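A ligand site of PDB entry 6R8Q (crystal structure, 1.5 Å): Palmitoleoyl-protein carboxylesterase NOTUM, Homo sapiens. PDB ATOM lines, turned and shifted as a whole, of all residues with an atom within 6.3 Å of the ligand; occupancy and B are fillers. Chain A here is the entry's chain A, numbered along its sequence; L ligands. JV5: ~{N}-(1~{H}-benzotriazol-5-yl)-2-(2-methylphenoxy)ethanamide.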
ATOM      1  N   GLY A  49      -4.598   6.250   6.790  1.00  0.00           N
ATOM      2  CA  GLY A  49      -5.604   6.964   6.022  1.00  0.00           C
ATOM      3  C   GLY A  49      -6.626   6.026   5.416  1.00  0.00           C
ATOM      4  O   GLY A  49      -6.670   4.831   5.721  1.00  0.00           O
ATOM      5  N   GLY A  50      -7.459   6.587   4.539  1.00  0.00           N
ATOM      6  CA  GLY A  50      -8.479   5.812   3.858  1.00  0.00           C
ATOM      7  C   GLY A  50      -9.806   6.528   3.649  1.00  0.00           C
ATOM      8  O   GLY A  50     -10.867   5.955   3.903  1.00  0.00           O
ATOM      9  N   TRP A  51      -9.769   7.768   3.164  1.00  0.00           N
ATOM     10  CA  TRP A  51     -10.994   8.523   2.816  1.00  0.00           C
ATOM     11  C   TRP A  51     -11.891   8.635   4.063  1.00  0.00           C
ATOM     12  O   TRP A  51     -11.388   8.813   5.175  1.00  0.00           O
ATOM     13  CB  TRP A  51     -11.647   8.000   1.538  1.00  0.00           C
ATOM     14  CG  TRP A  51     -12.263   9.086   0.690  1.00  0.00           C
ATOM     15  CD1 TRP A  51     -12.744  10.295   1.126  1.00  0.00           C
ATOM     16  CD2 TRP A  51     -12.429   9.090  -0.736  1.00  0.00           C
ATOM     17  NE1 TRP A  51     -13.205  11.035   0.063  1.00  0.00           N
ATOM     18  CE2 TRP A  51     -13.023  10.313  -1.093  1.00  0.00           C
ATOM     19  CE3 TRP A  51     -12.144   8.162  -1.743  1.00  0.00           C
ATOM     20  CZ2 TRP A  51     -13.335  10.645  -2.412  1.00  0.00           C
ATOM     21  CZ3 TRP A  51     -12.451   8.486  -3.067  1.00  0.00           C
ATOM     22  CH2 TRP A  51     -13.040   9.726  -3.380  1.00  0.00           C
ATOM     23  N   TYR A  52     -13.206   8.527   3.889  1.00  0.00           N
ATOM     24  CA  TYR A  52     -14.173   8.652   4.979  1.00  0.00           C
ATOM     25  C   TYR A  52     -15.523   8.253   4.407  1.00  0.00           C
ATOM     26  O   TYR A  52     -15.673   8.062   3.209  1.00  0.00           O
ATOM     27  CB  TYR A  52     -14.250  10.072   5.551  1.00  0.00           C
ATOM     28  CG  TYR A  52     -14.422  11.193   4.537  1.00  0.00           C
ATOM     29  CD1 TYR A  52     -15.638  11.408   3.899  1.00  0.00           C
ATOM     30  CD2 TYR A  52     -13.373  12.047   4.225  1.00  0.00           C
ATOM     31  CE1 TYR A  52     -15.800  12.423   2.972  1.00  0.00           C
ATOM     32  CE2 TYR A  52     -13.530  13.078   3.300  1.00  0.00           C
ATOM     33  CZ  TYR A  52     -14.742  13.259   2.674  1.00  0.00           C
ATOM     34  OH  TYR A  52     -14.903  14.278   1.764  1.00  0.00           O
ATOM     35  N   TYR A 105      -7.024   2.843  10.845  1.00  0.00           N
ATOM     36  CA  TYR A 105      -8.133   3.769  10.678  1.00  0.00           C
ATOM     37  C   TYR A 105      -9.384   2.930  10.498  1.00  0.00           C
ATOM     38  O   TYR A 105      -9.587   2.328   9.443  1.00  0.00           O
ATOM     39  CB  TYR A 105      -7.858   4.597   9.430  1.00  0.00           C
ATOM     40  CG  TYR A 105      -8.871   5.632   9.033  1.00  0.00           C
ATOM     41  CD1 TYR A 105      -9.475   6.471   9.980  1.00  0.00           C
ATOM     42  CD2 TYR A 105      -9.154   5.847   7.689  1.00  0.00           C
ATOM     43  CE1 TYR A 105     -10.371   7.456   9.574  1.00  0.00           C
ATOM     44  CE2 TYR A 105     -10.025   6.817   7.291  1.00  0.00           C
ATOM     45  CZ  TYR A 105     -10.640   7.624   8.233  1.00  0.00           C
ATOM     46  OH  TYR A 105     -11.490   8.612   7.829  1.00  0.00           O
ATOM     47  N   VAL A 110     -12.116  10.793   9.527  1.00  0.00           N
ATOM     48  CA  VAL A 110     -10.943  11.664   9.469  1.00  0.00           C
ATOM     49  C   VAL A 110     -10.381  11.845  10.871  1.00  0.00           C
ATOM     50  O   VAL A 110      -9.781  12.879  11.195  1.00  0.00           O
ATOM     51  CB  VAL A 110     -11.246  13.002   8.767  1.00  0.00           C
ATOM     52  CG1 VAL A 110      -9.967  13.651   8.275  1.00  0.00           C
ATOM     53  CG2 VAL A 110     -12.175  12.793   7.560  1.00  0.00           C
ATOM     54  N   SER A 155      -2.712  10.943   4.358  1.00  0.00           N
ATOM     55  CA  SER A 155      -4.018  11.178   3.740  1.00  0.00           C
ATOM     56  C   SER A 155      -5.022  11.574   4.823  1.00  0.00           C
ATOM     57  O   SER A 155      -4.742  12.543   5.554  1.00  0.00           O
ATOM     58  CB  SER A 155      -4.397  10.020   2.830  1.00  0.00           C
ATOM     59  OG  SER A 155      -5.551  10.375   2.088  1.00  0.00           O
ATOM     60  N   ALA A 156      -6.147  10.870   4.973  1.00  0.00           N
ATOM     61  CA  ALA A 156      -7.057  11.165   6.077  1.00  0.00           C
ATOM     62  C   ALA A 156      -6.334  11.111   7.417  1.00  0.00           C
ATOM     63  O   ALA A 156      -6.710  11.829   8.351  1.00  0.00           O
ATOM     64  CB  ALA A 156      -8.272  10.212   6.066  1.00  0.00           C
ATOM     65  N   GLY A 157      -5.298  10.278   7.534  1.00  0.00           N
ATOM     66  CA  GLY A 157      -4.506  10.273   8.747  1.00  0.00           C
ATOM     67  C   GLY A 157      -3.658  11.516   8.917  1.00  0.00           C
ATOM     68  O   GLY A 157      -3.351  11.914  10.055  1.00  0.00           O
ATOM     69  N   THR A 159      -4.627  14.580   7.841  1.00  0.00           N
ATOM     70  CA  THR A 159      -5.594  15.516   8.402  1.00  0.00           C
ATOM     71  C   THR A 159      -5.847  15.208   9.877  1.00  0.00           C
ATOM     72  O   THR A 159      -5.929  16.118  10.710  1.00  0.00           O
ATOM     73  CB  THR A 159      -6.904  15.464   7.601  1.00  0.00           C
ATOM     74  OG1 THR A 159      -6.609  15.535   6.189  1.00  0.00           O
ATOM     75  CG2 THR A 159      -7.808  16.633   7.961  1.00  0.00           C
ATOM     76  N   SER A 188       0.198  14.345   3.121  1.00  0.00           N
ATOM     77  CA  SER A 188      -0.873  14.228   2.129  1.00  0.00           C
ATOM     78  C   SER A 188      -2.261  14.473   2.713  1.00  0.00           C
ATOM     79  O   SER A 188      -3.258  13.926   2.237  1.00  0.00           O
ATOM     80  CB  SER A 188      -0.817  12.878   1.407  1.00  0.00           C
ATOM     81  OG  SER A 188       0.412  12.761   0.712  1.00  0.00           O
ATOM     82  N   GLY A 189      -2.330  15.287   3.766  1.00  0.00           N
ATOM     83  CA  GLY A 189      -3.602  15.633   4.363  1.00  0.00           C
ATOM     84  C   GLY A 189      -3.906  17.109   4.377  1.00  0.00           C
ATOM     85  O   GLY A 189      -4.766  17.555   5.139  1.00  0.00           O
ATOM     86  N   PHE A 191      -5.450  19.706   2.337  1.00  0.00           N
ATOM     87  CA  PHE A 191      -6.361  19.871   1.216  1.00  0.00           C
ATOM     88  C   PHE A 191      -6.813  21.324   1.086  1.00  0.00           C
ATOM     89  O   PHE A 191      -6.807  22.094   2.054  1.00  0.00           O
ATOM     90  CB  PHE A 191      -7.593  18.980   1.389  1.00  0.00           C
ATOM     91  CG  PHE A 191      -7.298  17.500   1.287  1.00  0.00           C
ATOM     92  CD1 PHE A 191      -6.966  16.775   2.421  1.00  0.00           C
ATOM     93  CD2 PHE A 191      -7.426  16.832   0.076  1.00  0.00           C
ATOM     94  CE1 PHE A 191      -6.700  15.412   2.345  1.00  0.00           C
ATOM     95  CE2 PHE A 191      -7.187  15.453  -0.008  1.00  0.00           C
ATOM     96  CZ  PHE A 191      -6.812  14.746   1.125  1.00  0.00           C
ATOM     97  N   LEU A 192      -7.220  21.685  -0.127  1.00  0.00           N
ATOM     98  CA  LEU A 192      -7.713  23.010  -0.447  1.00  0.00           C
ATOM     99  C   LEU A 192      -9.211  22.936  -0.699  1.00  0.00           C
ATOM    100  O   LEU A 192      -9.679  22.052  -1.423  1.00  0.00           O
ATOM    101  CB  LEU A 192      -7.018  23.577  -1.692  1.00  0.00           C
ATOM    102  CG  LEU A 192      -5.507  23.735  -1.595  1.00  0.00           C
ATOM    103  CD1 LEU A 192      -4.939  24.388  -2.856  1.00  0.00           C
ATOM    104  CD2 LEU A 192      -5.086  24.524  -0.315  1.00  0.00           C
ATOM    105  N   PRO A 210     -15.948  18.231  -1.029  1.00  0.00           N
ATOM    106  CA  PRO A 210     -15.457  17.992   0.342  1.00  0.00           C
ATOM    107  C   PRO A 210     -16.020  18.934   1.389  1.00  0.00           C
ATOM    108  O   PRO A 210     -16.344  18.479   2.486  1.00  0.00           O
ATOM    109  CB  PRO A 210     -13.942  18.136   0.212  1.00  0.00           C
ATOM    110  CG  PRO A 210     -13.644  17.832  -1.199  1.00  0.00           C
ATOM    111  CD  PRO A 210     -14.847  18.244  -2.014  1.00  0.00           C
ATOM    112  N   THR A 211     -16.123  20.225   1.097  1.00  0.00           N
ATOM    113  CA  THR A 211     -16.671  21.144   2.088  1.00  0.00           C
ATOM    114  C   THR A 211     -18.054  20.700   2.538  1.00  0.00           C
ATOM    115  O   THR A 211     -18.345  20.686   3.742  1.00  0.00           O
ATOM    116  CB  THR A 211     -16.714  22.570   1.552  1.00  0.00           C
ATOM    117  OG1 THR A 211     -17.451  22.607   0.328  1.00  0.00           O
ATOM    118  CG2 THR A 211     -15.312  23.096   1.314  1.00  0.00           C
ATOM    119  N   ILE A 214     -17.843  17.171   4.388  1.00  0.00           N
ATOM    120  CA  ILE A 214     -17.316  17.290   5.740  1.00  0.00           C
ATOM    121  C   ILE A 214     -18.312  17.980   6.661  1.00  0.00           C
ATOM    122  O   ILE A 214     -18.462  17.600   7.832  1.00  0.00           O
ATOM    123  CB  ILE A 214     -15.939  17.989   5.740  1.00  0.00           C
ATOM    124  CG1 ILE A 214     -14.878  17.072   5.128  1.00  0.00           C
ATOM    125  CG2 ILE A 214     -15.539  18.401   7.147  1.00  0.00           C
ATOM    126  CD1 ILE A 214     -13.699  17.822   4.628  1.00  0.00           C
ATOM    127  N   PHE A 242     -10.987  21.298   9.127  1.00  0.00           N
ATOM    128  CA  PHE A 242     -10.457  20.124   8.438  1.00  0.00           C
ATOM    129  C   PHE A 242      -9.502  20.504   7.308  1.00  0.00           C
ATOM    130  O   PHE A 242      -8.885  19.616   6.702  1.00  0.00           O
ATOM    131  CB  PHE A 242     -11.595  19.283   7.855  1.00  0.00           C
ATOM    132  CG  PHE A 242     -12.301  18.436   8.881  1.00  0.00           C
ATOM    133  CD1 PHE A 242     -13.023  19.009   9.915  1.00  0.00           C
ATOM    134  CD2 PHE A 242     -12.284  17.062   8.765  1.00  0.00           C
ATOM    135  CE1 PHE A 242     -13.680  18.220  10.844  1.00  0.00           C
ATOM    136  CE2 PHE A 242     -12.947  16.253   9.674  1.00  0.00           C
ATOM    137  CZ  PHE A 242     -13.636  16.837  10.727  1.00  0.00           C
ATOM    138  N   PHE A 243      -9.375  21.794   7.014  1.00  0.00           N
ATOM    139  CA  PHE A 243      -8.514  22.276   5.946  1.00  0.00           C
ATOM    140  C   PHE A 243      -7.221  22.794   6.551  1.00  0.00           C
ATOM    141  O   PHE A 243      -7.224  23.763   7.336  1.00  0.00           O
ATOM    142  CB  PHE A 243      -9.258  23.289   5.093  1.00  0.00           C
ATOM    143  CG  PHE A 243     -10.330  22.627   4.291  1.00  0.00           C
ATOM    144  CD1 PHE A 243     -10.048  22.162   3.022  1.00  0.00           C
ATOM    145  CD2 PHE A 243     -11.568  22.354   4.850  1.00  0.00           C
ATOM    146  CE1 PHE A 243     -11.003  21.495   2.290  1.00  0.00           C
ATOM    147  CE2 PHE A 243     -12.530  21.687   4.130  1.00  0.00           C
ATOM    148  CZ  PHE A 243     -12.238  21.252   2.848  1.00  0.00           C
ATOM    149  N   GLY A 244      -6.117  22.141   6.194  1.00  0.00           N
ATOM    150  CA  GLY A 244      -4.845  22.368   6.878  1.00  0.00           C
ATOM    151  C   GLY A 244      -4.455  23.826   6.968  1.00  0.00           C
ATOM    152  O   GLY A 244      -4.049  24.299   8.037  1.00  0.00           O
ATOM    153  N   GLU A 264      -2.992  13.569  -5.879  1.00  0.00           N
ATOM    154  CA  GLU A 264      -4.013  12.860  -6.639  1.00  0.00           C
ATOM    155  C   GLU A 264      -5.367  12.889  -5.947  1.00  0.00           C
ATOM    156  O   GLU A 264      -6.405  12.898  -6.631  1.00  0.00           O
ATOM    157  CB  GLU A 264      -3.571  11.419  -6.894  1.00  0.00           C
ATOM    158  CG  GLU A 264      -2.513  11.300  -7.980  1.00  0.00           C
ATOM    159  CD  GLU A 264      -1.771   9.980  -7.949  1.00  0.00           C
ATOM    160  OE1 GLU A 264      -1.823   9.288  -6.898  1.00  0.00           O
ATOM    161  OE2 GLU A 264      -1.129   9.638  -8.955  1.00  0.00           O
ATOM    162  N   ALA A 265      -5.402  12.883  -4.608  1.00  0.00           N
ATOM    163  CA  ALA A 265      -6.693  12.924  -3.928  1.00  0.00           C
ATOM    164  C   ALA A 265      -7.330  14.310  -4.074  1.00  0.00           C
ATOM    165  O   ALA A 265      -8.546  14.415  -4.252  1.00  0.00           O
ATOM    166  CB  ALA A 265      -6.547  12.541  -2.458  1.00  0.00           C
ATOM    167  N   GLN A 266      -6.510  15.356  -4.015  1.00  0.00           N
ATOM    168  CA  GLN A 266      -7.002  16.709  -4.270  1.00  0.00           C
ATOM    169  C   GLN A 266      -7.583  16.810  -5.677  1.00  0.00           C
ATOM    170  O   GLN A 266      -8.675  17.360  -5.867  1.00  0.00           O
ATOM    171  CB  GLN A 266      -5.842  17.702  -4.105  1.00  0.00           C
ATOM    172  CG  GLN A 266      -6.223  19.163  -4.384  1.00  0.00           C
ATOM    173  CD  GLN A 266      -7.057  19.782  -3.287  1.00  0.00           C
ATOM    174  OE1 GLN A 266      -6.714  19.703  -2.106  1.00  0.00           O
ATOM    175  NE2 GLN A 266      -8.187  20.395  -3.677  1.00  0.00           N
ATOM    176  N   THR A 268      -8.740  14.389  -7.514  1.00  0.00           N
ATOM    177  CA  THR A 268      -9.974  13.605  -7.546  1.00  0.00           C
ATOM    178  C   THR A 268     -11.149  14.403  -7.003  1.00  0.00           C
ATOM    179  O   THR A 268     -12.222  14.439  -7.619  1.00  0.00           O
ATOM    180  CB  THR A 268      -9.772  12.323  -6.744  1.00  0.00           C
ATOM    181  OG1 THR A 268      -8.844  11.476  -7.414  1.00  0.00           O
ATOM    182  CG2 THR A 268     -11.106  11.597  -6.551  1.00  0.00           C
ATOM    183  N   VAL A 269     -10.973  15.036  -5.834  1.00  0.00           N
ATOM    184  CA  VAL A 269     -12.078  15.823  -5.281  1.00  0.00           C
ATOM    185  C   VAL A 269     -12.343  17.092  -6.071  1.00  0.00           C
ATOM    186  O   VAL A 269     -13.418  17.672  -5.932  1.00  0.00           O
ATOM    187  CB  VAL A 269     -11.957  16.041  -3.756  1.00  0.00           C
ATOM    188  CG1 VAL A 269     -11.779  14.711  -3.030  1.00  0.00           C
ATOM    189  CG2 VAL A 269     -10.821  17.009  -3.430  1.00  0.00           C
ATOM    190  N   HIS A 312       0.350  10.594  -4.246  1.00  0.00           N
ATOM    191  CA  HIS A 312      -0.443  10.657  -3.025  1.00  0.00           C
ATOM    192  C   HIS A 312       0.225   9.777  -1.970  1.00  0.00           C
ATOM    193  O   HIS A 312       0.485   8.599  -2.226  1.00  0.00           O
ATOM    194  CB  HIS A 312      -1.883  10.173  -3.290  1.00  0.00           C
ATOM    195  CG  HIS A 312      -2.812  10.367  -2.116  1.00  0.00           C
ATOM    196  ND1 HIS A 312      -2.940  11.565  -1.453  1.00  0.00           N
ATOM    197  CD2 HIS A 312      -3.630   9.492  -1.484  1.00  0.00           C
ATOM    198  CE1 HIS A 312      -3.810  11.439  -0.471  1.00  0.00           C
ATOM    199  NE2 HIS A 312      -4.252  10.187  -0.465  1.00  0.00           N
HETATM  200  C4  JV5 L   1      -9.910  17.190   4.846  1.00  0.00           C
HETATM  201  C5  JV5 L   1      -9.868  15.867   4.469  1.00  0.00           C
HETATM  202  C6  JV5 L   1     -10.263  15.517   3.185  1.00  0.00           C
HETATM  203  C7  JV5 L   1      -9.521  13.250   3.383  1.00  0.00           C
HETATM  204  C8  JV5 L   1      -9.299  12.110   2.418  1.00  0.00           C
HETATM  205  C10 JV5 L   1     -10.032  12.071  -1.213  1.00  0.00           C
HETATM  206  C13 JV5 L   1      -8.764   9.615  -1.176  1.00  0.00           C
HETATM  207  C1  JV5 L   1     -10.690  16.476   2.269  1.00  0.00           C
HETATM  208  C2  JV5 L   1     -10.739  17.798   2.682  1.00  0.00           C
HETATM  209  C3  JV5 L   1     -10.347  18.161   3.963  1.00  0.00           C
HETATM  210  C9  JV5 L   1      -9.523  11.567  -0.013  1.00  0.00           C
HETATM  211  C12 JV5 L   1      -9.264  10.121  -2.371  1.00  0.00           C
HETATM  212  N   JV5 L   1      -9.682  12.361   1.144  1.00  0.00           N
HETATM  213  C   JV5 L   1     -11.012  16.098   0.832  1.00  0.00           C
HETATM  214  O   JV5 L   1     -10.265  14.242   2.688  1.00  0.00           O
HETATM  215  C11 JV5 L   1      -9.905  11.363  -2.386  1.00  0.00           C
HETATM  216  C14 JV5 L   1      -8.890  10.326   0.014  1.00  0.00           C
HETATM  217  N1  JV5 L   1      -9.011   9.209  -3.374  1.00  0.00           N
HETATM  218  N2  JV5 L   1      -8.394   8.194  -2.843  1.00  0.00           N
HETATM  219  N3  JV5 L   1      -8.228   8.413  -1.522  1.00  0.00           N
HETATM  220  O1  JV5 L   1      -8.795  11.065   2.809  1.00  0.00           O
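Residues that only touch the ligand: Tyr 52 (3.5 Å), Thr 159 (3.7 Å), Phe 191 (3.6 Å), Pro 210 (3.6 Å), Ile 214 (3.4 Å), Phe 242 (3.2 Å), Phe 243 (3.7 Å), Ala 265 (3.6 Å) and Val 269 (3.7 Å). 12 residues have an atom within 4 Å of the ligand: Trp 51, Tyr 52, Ser 155, Ala 156, Thr 159, Phe 191, Pro 210, Ile 214, Phe 242, Phe 243, Ala 265 and Val 269. Along chain A the residues within 4 Å of the ligand span positions 51 to 269.
The side-chain hydroxyl of Tyr 105 lies within hydrogen-bond range of the backbone carbonyl oxygen of Trp 51, at 2.7 Å. The side-chain hydroxyl (OG) of Ser 155 sits at hydrogen-bond distance from a ring nitrogen (NE2) of His 312 (2.9 Å). The side-chain hydroxyl (OG1) of Thr 159 is in hydrogen-bond range of the backbone carbonyl oxygen (O) of Gly 189 (2.9 Å).
N of Trp 51 sits close to O1 of the ligand, 3.5 Å away. OG of Ser 155 sits at hydrogen-bond distance from O1 of the ligand, at 3.4 Å. The backbone NH of Ala 156 lies close to an oxygen (O1) of the ligand, 3.4 Å away.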
